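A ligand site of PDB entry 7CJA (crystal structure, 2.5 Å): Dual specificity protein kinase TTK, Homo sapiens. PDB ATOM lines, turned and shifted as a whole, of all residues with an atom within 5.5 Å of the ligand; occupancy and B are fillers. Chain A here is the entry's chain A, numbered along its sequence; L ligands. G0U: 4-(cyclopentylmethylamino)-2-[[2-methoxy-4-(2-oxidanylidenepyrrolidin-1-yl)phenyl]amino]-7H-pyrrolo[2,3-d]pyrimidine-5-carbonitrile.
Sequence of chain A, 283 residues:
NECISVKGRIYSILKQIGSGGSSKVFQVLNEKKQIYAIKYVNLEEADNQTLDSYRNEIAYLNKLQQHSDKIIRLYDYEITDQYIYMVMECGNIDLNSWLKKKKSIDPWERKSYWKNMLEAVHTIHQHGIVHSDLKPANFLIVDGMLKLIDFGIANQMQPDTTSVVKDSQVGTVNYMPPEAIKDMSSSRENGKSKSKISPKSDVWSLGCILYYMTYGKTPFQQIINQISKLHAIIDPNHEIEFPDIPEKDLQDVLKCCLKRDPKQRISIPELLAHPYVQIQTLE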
ATOM      1  N   LYS A  15     -31.439  12.320 -10.694  1.00  0.00           N
ATOM      2  CA  LYS A  15     -31.384  10.920 -10.328  1.00  0.00           C
ATOM      3  C   LYS A  15     -30.188  10.726  -9.415  1.00  0.00           C
ATOM      4  O   LYS A  15     -29.374  11.619  -9.226  1.00  0.00           O
ATOM      5  CB  LYS A  15     -31.289  10.031 -11.573  1.00  0.00           C
ATOM      6  CG  LYS A  15     -29.920  10.021 -12.242  1.00  0.00           C
ATOM      7  CD  LYS A  15     -30.032   9.620 -13.685  1.00  0.00           C
ATOM      8  CE  LYS A  15     -28.901   8.711 -14.139  1.00  0.00           C
ATOM      9  NZ  LYS A  15     -29.367   7.299 -14.228  1.00  0.00           N
ATOM     10  N   ILE A  17     -26.767   8.894  -9.125  1.00  0.00           N
ATOM     11  CA  ILE A  17     -25.757   8.233  -9.935  1.00  0.00           C
ATOM     12  C   ILE A  17     -25.070   7.123  -9.158  1.00  0.00           C
ATOM     13  O   ILE A  17     -24.648   6.118  -9.747  1.00  0.00           O
ATOM     14  CB  ILE A  17     -24.707   9.247 -10.401  1.00  0.00           C
ATOM     15  CG1 ILE A  17     -25.288  10.372 -11.241  1.00  0.00           C
ATOM     16  CG2 ILE A  17     -23.577   8.526 -11.128  1.00  0.00           C
ATOM     17  CD1 ILE A  17     -24.221  11.488 -11.434  1.00  0.00           C
ATOM     18  N   GLY A  18     -24.833   7.322  -7.859  1.00  0.00           N
ATOM     19  CA  GLY A  18     -23.921   6.392  -7.197  1.00  0.00           C
ATOM     20  C   GLY A  18     -23.956   6.481  -5.690  1.00  0.00           C
ATOM     21  O   GLY A  18     -24.527   7.402  -5.105  1.00  0.00           O
ATOM     22  N   VAL A  25     -24.121  10.001  -4.602  1.00  0.00           N
ATOM     23  CA  VAL A  25     -23.923  10.983  -5.671  1.00  0.00           C
ATOM     24  C   VAL A  25     -25.210  11.102  -6.474  1.00  0.00           C
ATOM     25  O   VAL A  25     -25.774  10.098  -6.914  1.00  0.00           O
ATOM     26  CB  VAL A  25     -22.761  10.621  -6.607  1.00  0.00           C
ATOM     27  CG1 VAL A  25     -22.391  11.849  -7.403  1.00  0.00           C
ATOM     28  CG2 VAL A  25     -21.575  10.109  -5.831  1.00  0.00           C
ATOM     29  N   GLN A  27     -27.084  13.202  -9.773  1.00  0.00           N
ATOM     30  CA  GLN A  27     -27.139  14.152 -10.876  1.00  0.00           C
ATOM     31  C   GLN A  27     -28.246  15.160 -10.598  1.00  0.00           C
ATOM     32  O   GLN A  27     -29.393  14.761 -10.348  1.00  0.00           O
ATOM     33  CB  GLN A  27     -27.364  13.407 -12.191  1.00  0.00           C
ATOM     34  CG  GLN A  27     -27.582  14.268 -13.436  1.00  0.00           C
ATOM     35  CD  GLN A  27     -27.849  13.410 -14.682  1.00  0.00           C
ATOM     36  OE1 GLN A  27     -27.160  13.532 -15.694  1.00  0.00           O
ATOM     37  NE2 GLN A  27     -28.826  12.510 -14.591  1.00  0.00           N
ATOM     38  N   ALA A  37     -23.065  17.439 -10.492  1.00  0.00           N
ATOM     39  CA  ALA A  37     -23.144  16.314  -9.565  1.00  0.00           C
ATOM     40  C   ALA A  37     -23.110  16.865  -8.139  1.00  0.00           C
ATOM     41  O   ALA A  37     -22.493  17.905  -7.878  1.00  0.00           O
ATOM     42  CB  ALA A  37     -22.008  15.305  -9.786  1.00  0.00           C
ATOM     43  N   LYS A  39     -22.263  15.170  -4.354  1.00  0.00           N
ATOM     44  CA  LYS A  39     -21.972  14.094  -3.430  1.00  0.00           C
ATOM     45  C   LYS A  39     -22.471  14.483  -2.031  1.00  0.00           C
ATOM     46  O   LYS A  39     -22.222  15.596  -1.557  1.00  0.00           O
ATOM     47  CB  LYS A  39     -20.463  13.788  -3.432  1.00  0.00           C
ATOM     48  CG  LYS A  39     -20.031  12.536  -2.680  1.00  0.00           C
ATOM     49  CD  LYS A  39     -18.540  12.306  -2.819  1.00  0.00           C
ATOM     50  CE  LYS A  39     -18.096  11.105  -2.011  1.00  0.00           C
ATOM     51  NZ  LYS A  39     -16.650  10.768  -2.194  1.00  0.00           N
ATOM     52  N   ILE A  72     -11.623  16.329 -12.082  1.00  0.00           N
ATOM     53  CA  ILE A  72     -13.012  16.722 -11.868  1.00  0.00           C
ATOM     54  C   ILE A  72     -13.088  17.878 -10.874  1.00  0.00           C
ATOM     55  O   ILE A  72     -12.487  17.822  -9.792  1.00  0.00           O
ATOM     56  CB  ILE A  72     -13.822  15.519 -11.385  1.00  0.00           C
ATOM     57  CG1 ILE A  72     -15.248  15.576 -11.925  1.00  0.00           C
ATOM     58  CG2 ILE A  72     -13.808  15.492  -9.866  1.00  0.00           C
ATOM     59  CD1 ILE A  72     -15.363  15.073 -13.403  1.00  0.00           C
ATOM     60  N   MET A  88     -20.133  19.385  -7.689  1.00  0.00           N
ATOM     61  CA  MET A  88     -19.030  19.092  -8.582  1.00  0.00           C
ATOM     62  C   MET A  88     -19.440  19.067 -10.044  1.00  0.00           C
ATOM     63  O   MET A  88     -20.613  18.923 -10.405  1.00  0.00           O
ATOM     64  CB  MET A  88     -18.379  17.752  -8.272  1.00  0.00           C
ATOM     65  CG  MET A  88     -17.824  17.678  -6.856  1.00  0.00           C
ATOM     66  SD  MET A  88     -17.658  15.983  -6.289  1.00  0.00           S
ATOM     67  CE  MET A  88     -15.985  15.722  -6.828  1.00  0.00           C
ATOM     68  N   GLU A  89     -18.415  19.209 -10.895  1.00  0.00           N
ATOM     69  CA  GLU A  89     -18.566  18.965 -12.316  1.00  0.00           C
ATOM     70  C   GLU A  89     -19.184  17.595 -12.522  1.00  0.00           C
ATOM     71  O   GLU A  89     -18.740  16.606 -11.912  1.00  0.00           O
ATOM     72  CB  GLU A  89     -17.183  19.065 -12.969  1.00  0.00           C
ATOM     73  CG  GLU A  89     -17.057  18.536 -14.401  1.00  0.00           C
ATOM     74  CD  GLU A  89     -15.740  18.926 -15.046  1.00  0.00           C
ATOM     75  OE1 GLU A  89     -15.745  19.352 -16.216  1.00  0.00           O
ATOM     76  OE2 GLU A  89     -14.693  18.828 -14.364  1.00  0.00           O
ATOM     77  N   CYS A  90     -20.242  17.507 -13.312  1.00  0.00           N
ATOM     78  CA  CYS A  90     -20.929  16.237 -13.493  1.00  0.00           C
ATOM     79  C   CYS A  90     -20.419  15.551 -14.758  1.00  0.00           C
ATOM     80  O   CYS A  90     -20.417  16.142 -15.842  1.00  0.00           O
ATOM     81  CB  CYS A  90     -22.445  16.419 -13.547  1.00  0.00           C
ATOM     82  SG  CYS A  90     -23.358  14.879 -13.605  1.00  0.00           S
ATOM     83  N   GLY A  91     -19.998  14.309 -14.628  1.00  0.00           N
ATOM     84  CA  GLY A  91     -19.619  13.552 -15.791  1.00  0.00           C
ATOM     85  C   GLY A  91     -20.823  13.028 -16.569  1.00  0.00           C
ATOM     86  O   GLY A  91     -21.932  12.871 -16.018  1.00  0.00           O
ATOM     87  N   ASN A  92     -20.596  12.747 -17.859  1.00  0.00           N
ATOM     88  CA  ASN A  92     -21.582  12.015 -18.649  1.00  0.00           C
ATOM     89  C   ASN A  92     -21.792  10.615 -18.116  1.00  0.00           C
ATOM     90  O   ASN A  92     -22.927  10.149 -17.954  1.00  0.00           O
ATOM     91  CB  ASN A  92     -21.143  11.932 -20.118  1.00  0.00           C
ATOM     92  CG  ASN A  92     -20.745  13.259 -20.690  1.00  0.00           C
ATOM     93  OD1 ASN A  92     -21.160  14.309 -20.202  1.00  0.00           O
ATOM     94  ND2 ASN A  92     -19.925  13.233 -21.728  1.00  0.00           N
ATOM     95  N   ILE A  93     -20.698   9.917 -17.848  1.00  0.00           N
ATOM     96  CA  ILE A  93     -20.683   8.514 -17.445  1.00  0.00           C
ATOM     97  C   ILE A  93     -19.247   8.228 -17.020  1.00  0.00           C
ATOM     98  O   ILE A  93     -18.345   9.015 -17.332  1.00  0.00           O
ATOM     99  CB  ILE A  93     -21.130   7.591 -18.601  1.00  0.00           C
ATOM    100  CG1 ILE A  93     -21.334   6.169 -18.085  1.00  0.00           C
ATOM    101  CG2 ILE A  93     -20.116   7.639 -19.734  1.00  0.00           C
ATOM    102  CD1 ILE A  93     -21.771   5.199 -19.154  1.00  0.00           C
ATOM    103  N   ASP A  94     -19.012   7.148 -16.286  1.00  0.00           N
ATOM    104  CA  ASP A  94     -17.649   6.807 -15.932  1.00  0.00           C
ATOM    105  C   ASP A  94     -17.050   5.860 -16.965  1.00  0.00           C
ATOM    106  O   ASP A  94     -17.759   5.112 -17.639  1.00  0.00           O
ATOM    107  CB  ASP A  94     -17.591   6.152 -14.561  1.00  0.00           C
ATOM    108  CG  ASP A  94     -18.267   4.850 -14.557  1.00  0.00           C
ATOM    109  OD1 ASP A  94     -19.459   4.911 -14.882  1.00  0.00           O
ATOM    110  OD2 ASP A  94     -17.652   3.794 -14.282  1.00  0.00           O
ATOM    111  N   SER A  97     -18.071   2.077 -16.975  1.00  0.00           N
ATOM    112  CA  SER A  97     -19.371   1.804 -17.590  1.00  0.00           C
ATOM    113  C   SER A  97     -19.322   1.975 -19.096  1.00  0.00           C
ATOM    114  O   SER A  97     -19.978   1.239 -19.836  1.00  0.00           O
ATOM    115  CB  SER A  97     -20.478   2.695 -17.024  1.00  0.00           C
ATOM    116  OG  SER A  97     -20.552   2.592 -15.615  1.00  0.00           O
ATOM    117  N   ALA A 137     -13.016   3.225 -13.329  1.00  0.00           N
ATOM    118  CA  ALA A 137     -14.072   3.936 -12.622  1.00  0.00           C
ATOM    119  C   ALA A 137     -13.605   5.270 -12.073  1.00  0.00           C
ATOM    120  O   ALA A 137     -14.449   6.128 -11.771  1.00  0.00           O
ATOM    121  CB  ALA A 137     -14.626   3.080 -11.474  1.00  0.00           C
ATOM    122  N   LEU A 140     -14.036  10.020 -15.474  1.00  0.00           N
ATOM    123  CA  LEU A 140     -15.319  10.373 -16.024  1.00  0.00           C
ATOM    124  C   LEU A 140     -15.107  11.089 -17.346  1.00  0.00           C
ATOM    125  O   LEU A 140     -14.146  11.837 -17.505  1.00  0.00           O
ATOM    126  CB  LEU A 140     -16.121  11.308 -15.082  1.00  0.00           C
ATOM    127  CG  LEU A 140     -16.280  10.854 -13.631  1.00  0.00           C
ATOM    128  CD1 LEU A 140     -17.086  11.879 -12.733  1.00  0.00           C
ATOM    129  CD2 LEU A 140     -16.884   9.464 -13.608  1.00  0.00           C
ATOM    130  N   ILE A 149     -11.531  11.357 -10.696  1.00  0.00           N
ATOM    131  CA  ILE A 149     -12.535  11.695  -9.675  1.00  0.00           C
ATOM    132  C   ILE A 149     -12.134  11.235  -8.267  1.00  0.00           C
ATOM    133  O   ILE A 149     -12.227  12.019  -7.309  1.00  0.00           O
ATOM    134  CB  ILE A 149     -13.961  11.206 -10.060  1.00  0.00           C
ATOM    135  CG1 ILE A 149     -14.924  11.515  -8.918  1.00  0.00           C
ATOM    136  CG2 ILE A 149     -14.050   9.711 -10.335  1.00  0.00           C
ATOM    137  CD1 ILE A 149     -14.845  12.932  -8.421  1.00  0.00           C
ATOM    138  N   ASP A 150     -11.759   9.961  -8.089  1.00  0.00           N
ATOM    139  CA  ASP A 150     -11.529   9.437  -6.730  1.00  0.00           C
ATOM    140  C   ASP A 150     -10.039   9.174  -6.514  1.00  0.00           C
ATOM    141  O   ASP A 150      -9.483   8.235  -7.093  1.00  0.00           O
ATOM    142  CB  ASP A 150     -12.325   8.150  -6.485  1.00  0.00           C
ATOM    143  CG  ASP A 150     -13.849   8.387  -6.273  1.00  0.00           C
ATOM    144  OD1 ASP A 150     -14.263   9.421  -5.695  1.00  0.00           O
ATOM    145  OD2 ASP A 150     -14.647   7.502  -6.687  1.00  0.00           O
ATOM    146  N   MET A 157     -16.753   5.172  -4.724  1.00  0.00           N
ATOM    147  CA  MET A 157     -18.168   5.041  -4.965  1.00  0.00           C
ATOM    148  C   MET A 157     -18.462   3.936  -5.988  1.00  0.00           C
ATOM    149  O   MET A 157     -17.597   3.535  -6.768  1.00  0.00           O
ATOM    150  CB  MET A 157     -18.732   6.362  -5.465  1.00  0.00           C
ATOM    151  CG  MET A 157     -18.701   7.458  -4.427  1.00  0.00           C
ATOM    152  SD  MET A 157     -20.069   7.198  -3.288  1.00  0.00           S
ATOM    153  CE  MET A 157     -20.677   8.871  -3.095  1.00  0.00           C
ATOM    154  N   GLN A 158     -19.698   3.455  -5.969  1.00  0.00           N
ATOM    155  CA  GLN A 158     -20.151   2.472  -6.933  1.00  0.00           C
ATOM    156  C   GLN A 158     -21.403   2.975  -7.639  1.00  0.00           C
ATOM    157  O   GLN A 158     -22.220   3.674  -7.022  1.00  0.00           O
ATOM    158  CB  GLN A 158     -20.449   1.119  -6.247  1.00  0.00           C
ATOM    159  CG  GLN A 158     -19.188   0.403  -5.747  1.00  0.00           C
ATOM    160  CD  GLN A 158     -18.330  -0.155  -6.879  1.00  0.00           C
ATOM    161  OE1 GLN A 158     -18.695  -0.060  -8.057  1.00  0.00           O
ATOM    162  NE2 GLN A 158     -17.189  -0.743  -6.523  1.00  0.00           N
ATOM    163  N   PRO A 159     -21.581   2.650  -8.922  1.00  0.00           N
ATOM    164  CA  PRO A 159     -22.738   3.170  -9.663  1.00  0.00           C
ATOM    165  C   PRO A 159     -24.021   2.461  -9.278  1.00  0.00           C
ATOM    166  O   PRO A 159     -24.024   1.267  -8.960  1.00  0.00           O
ATOM    167  CB  PRO A 159     -22.371   2.895 -11.111  1.00  0.00           C
ATOM    168  CG  PRO A 159     -21.515   1.681 -11.031  1.00  0.00           C
ATOM    169  CD  PRO A 159     -20.738   1.775  -9.752  1.00  0.00           C
ATOM    170  N   ASP A 160     -25.125   3.201  -9.324  1.00  0.00           N
ATOM    171  CA  ASP A 160     -26.449   2.631  -9.060  1.00  0.00           C
ATOM    172  C   ASP A 160     -27.209   2.313 -10.352  1.00  0.00           C
ATOM    173  O   ASP A 160     -26.897   2.848 -11.423  1.00  0.00           O
ATOM    174  CB  ASP A 160     -27.274   3.585  -8.208  1.00  0.00           C
ATOM    175  CG  ASP A 160     -26.724   3.742  -6.806  1.00  0.00           C
ATOM    176  OD1 ASP A 160     -25.907   2.894  -6.351  1.00  0.00           O
ATOM    177  OD2 ASP A 160     -27.095   4.735  -6.138  1.00  0.00           O
HETATM  178  C10 G0U L   1     -18.803  12.775  -9.026  1.00  0.00           C
HETATM  179  N12 G0U L   1     -18.994  14.280 -10.633  1.00  0.00           N
HETATM  180  C13 G0U L   1     -18.455  12.114  -7.710  1.00  0.00           C
HETATM  181  C15 G0U L   1     -20.019  10.923 -10.380  1.00  0.00           C
HETATM  182  C17 G0U L   1     -20.412   8.547 -10.029  1.00  0.00           C
HETATM  183  C20 G0U L   1     -18.687   5.445 -10.631  1.00  0.00           C
HETATM  184  C21 G0U L   1     -17.533   6.348  -9.859  1.00  0.00           C
HETATM  185  C22 G0U L   1     -18.057   7.599  -9.838  1.00  0.00           C
HETATM  186  C24 G0U L   1     -21.108   8.787 -13.741  1.00  0.00           C
HETATM  187  C26 G0U L   1     -23.007   7.517 -14.504  1.00  0.00           C
HETATM  188  C01 G0U L   1     -24.922  11.030 -15.419  1.00  0.00           C
HETATM  189  C03 G0U L   1     -23.126   9.894 -14.414  1.00  0.00           C
HETATM  190  C04 G0U L   1     -21.847   9.951 -13.941  1.00  0.00           C
HETATM  191  C06 G0U L   1     -20.704  11.646 -12.461  1.00  0.00           C
HETATM  192  C08 G0U L   1     -19.597  13.138 -11.087  1.00  0.00           C
HETATM  193  C09 G0U L   1     -19.479  12.185 -10.099  1.00  0.00           C
HETATM  194  C11 G0U L   1     -18.521  14.085  -9.396  1.00  0.00           C
HETATM  195  C18 G0U L   1     -19.596   7.379  -9.519  1.00  0.00           C
HETATM  196  C19 G0U L   1     -19.900   5.996 -10.287  1.00  0.00           C
HETATM  197  C25 G0U L   1     -21.690   7.550 -14.022  1.00  0.00           C
HETATM  198  C27 G0U L   1     -23.714   8.688 -14.700  1.00  0.00           C
HETATM  199  C29 G0U L   1     -23.133   4.827 -14.364  1.00  0.00           C
HETATM  200  C30 G0U L   1     -23.725   3.888 -15.186  1.00  0.00           C
HETATM  201  C31 G0U L   1     -25.040   4.520 -15.658  1.00  0.00           C
HETATM  202  C32 G0U L   1     -24.773   6.094 -15.610  1.00  0.00           C
HETATM  203  N05 G0U L   1     -21.357  11.297 -13.702  1.00  0.00           N
HETATM  204  N07 G0U L   1     -20.216  12.838 -12.273  1.00  0.00           N
HETATM  205  N14 G0U L   1     -18.202  11.620  -6.730  1.00  0.00           N
HETATM  206  N16 G0U L   1     -20.007   9.809  -9.456  1.00  0.00           N
HETATM  207  N23 G0U L   1     -20.612  10.722 -11.553  1.00  0.00           N
HETATM  208  N28 G0U L   1     -23.647   6.255 -14.830  1.00  0.00           N
HETATM  209  O02 G0U L   1     -23.784  11.099 -14.614  1.00  0.00           O
HETATM  210  O33 G0U L   1     -25.431   6.930 -16.147  1.00  0.00           O
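A nitrogen (N07) of the ligand is in hydrogen-bond range of the backbone NH (N) of Gly 91, 2.8 Å away.
N12 of the ligand is in hydrogen-bond range of O of Glu 89 (2.7 Å).
A nitrogen (N05) of the ligand is in hydrogen-bond range of the backbone carbonyl oxygen (O) of Gly 91.
Merely in contact with the ligand: Ile 17 (3.2 Å), Val 25 (3.7 Å), Gln 27 (3.4 Å), Ala 37 (3.3 Å), Lys 39 (3.99 Å), Met 88 (3.7 Å), Cys 90 (3.7 Å), Asn 92 (3.3 Å), Ile 93 (3.7 Å), Asp 94 (3.5 Å), Ser 97 (3.5 Å), Ala 137 (3.6 Å), Leu 140 (3.3 Å), Ile 149 (3.8 Å) and Pro 159 (3.9 Å).
Hydrophobic or aromatic side chains that line the ligand: Ile 17, Val 25, Ala 37, Met 88, Ile 93, Leu 140, Ile 149 and Pro 159.
17 residues have an atom within 4 Å of the ligand: Ile 17, Val 25, Gln 27, Ala 37, Lys 39, Met 88, Glu 89, Cys 90, Gly 91, Asn 92, Ile 93, Asp 94, Ser 97, Ala 137, Leu 140, Ile 149 and Pro 159.
N of Asp 160 sits at hydrogen-bond distance from O of Ile 17 (3.0 Å).
The backbone NH (N) of Met 88 lies within hydrogen-bond range of the backbone carbonyl oxygen (O) of Ala 37, at 2.8 Å.
N of Val 25 sits at hydrogen-bond distance from O of Gly 18 (2.7 Å).
The side-chain hydroxyl (OG) of Ser 97 is in hydrogen-bond range of the side-chain carboxylate (OD1) of Asp 94.
The backbone NH (N) of Ile 17 is in hydrogen-bond range of the backbone carbonyl oxygen (O) of Val 25.
N of Gln 27 is in hydrogen-bond range of O of Lys 15, 2.8 Å away.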
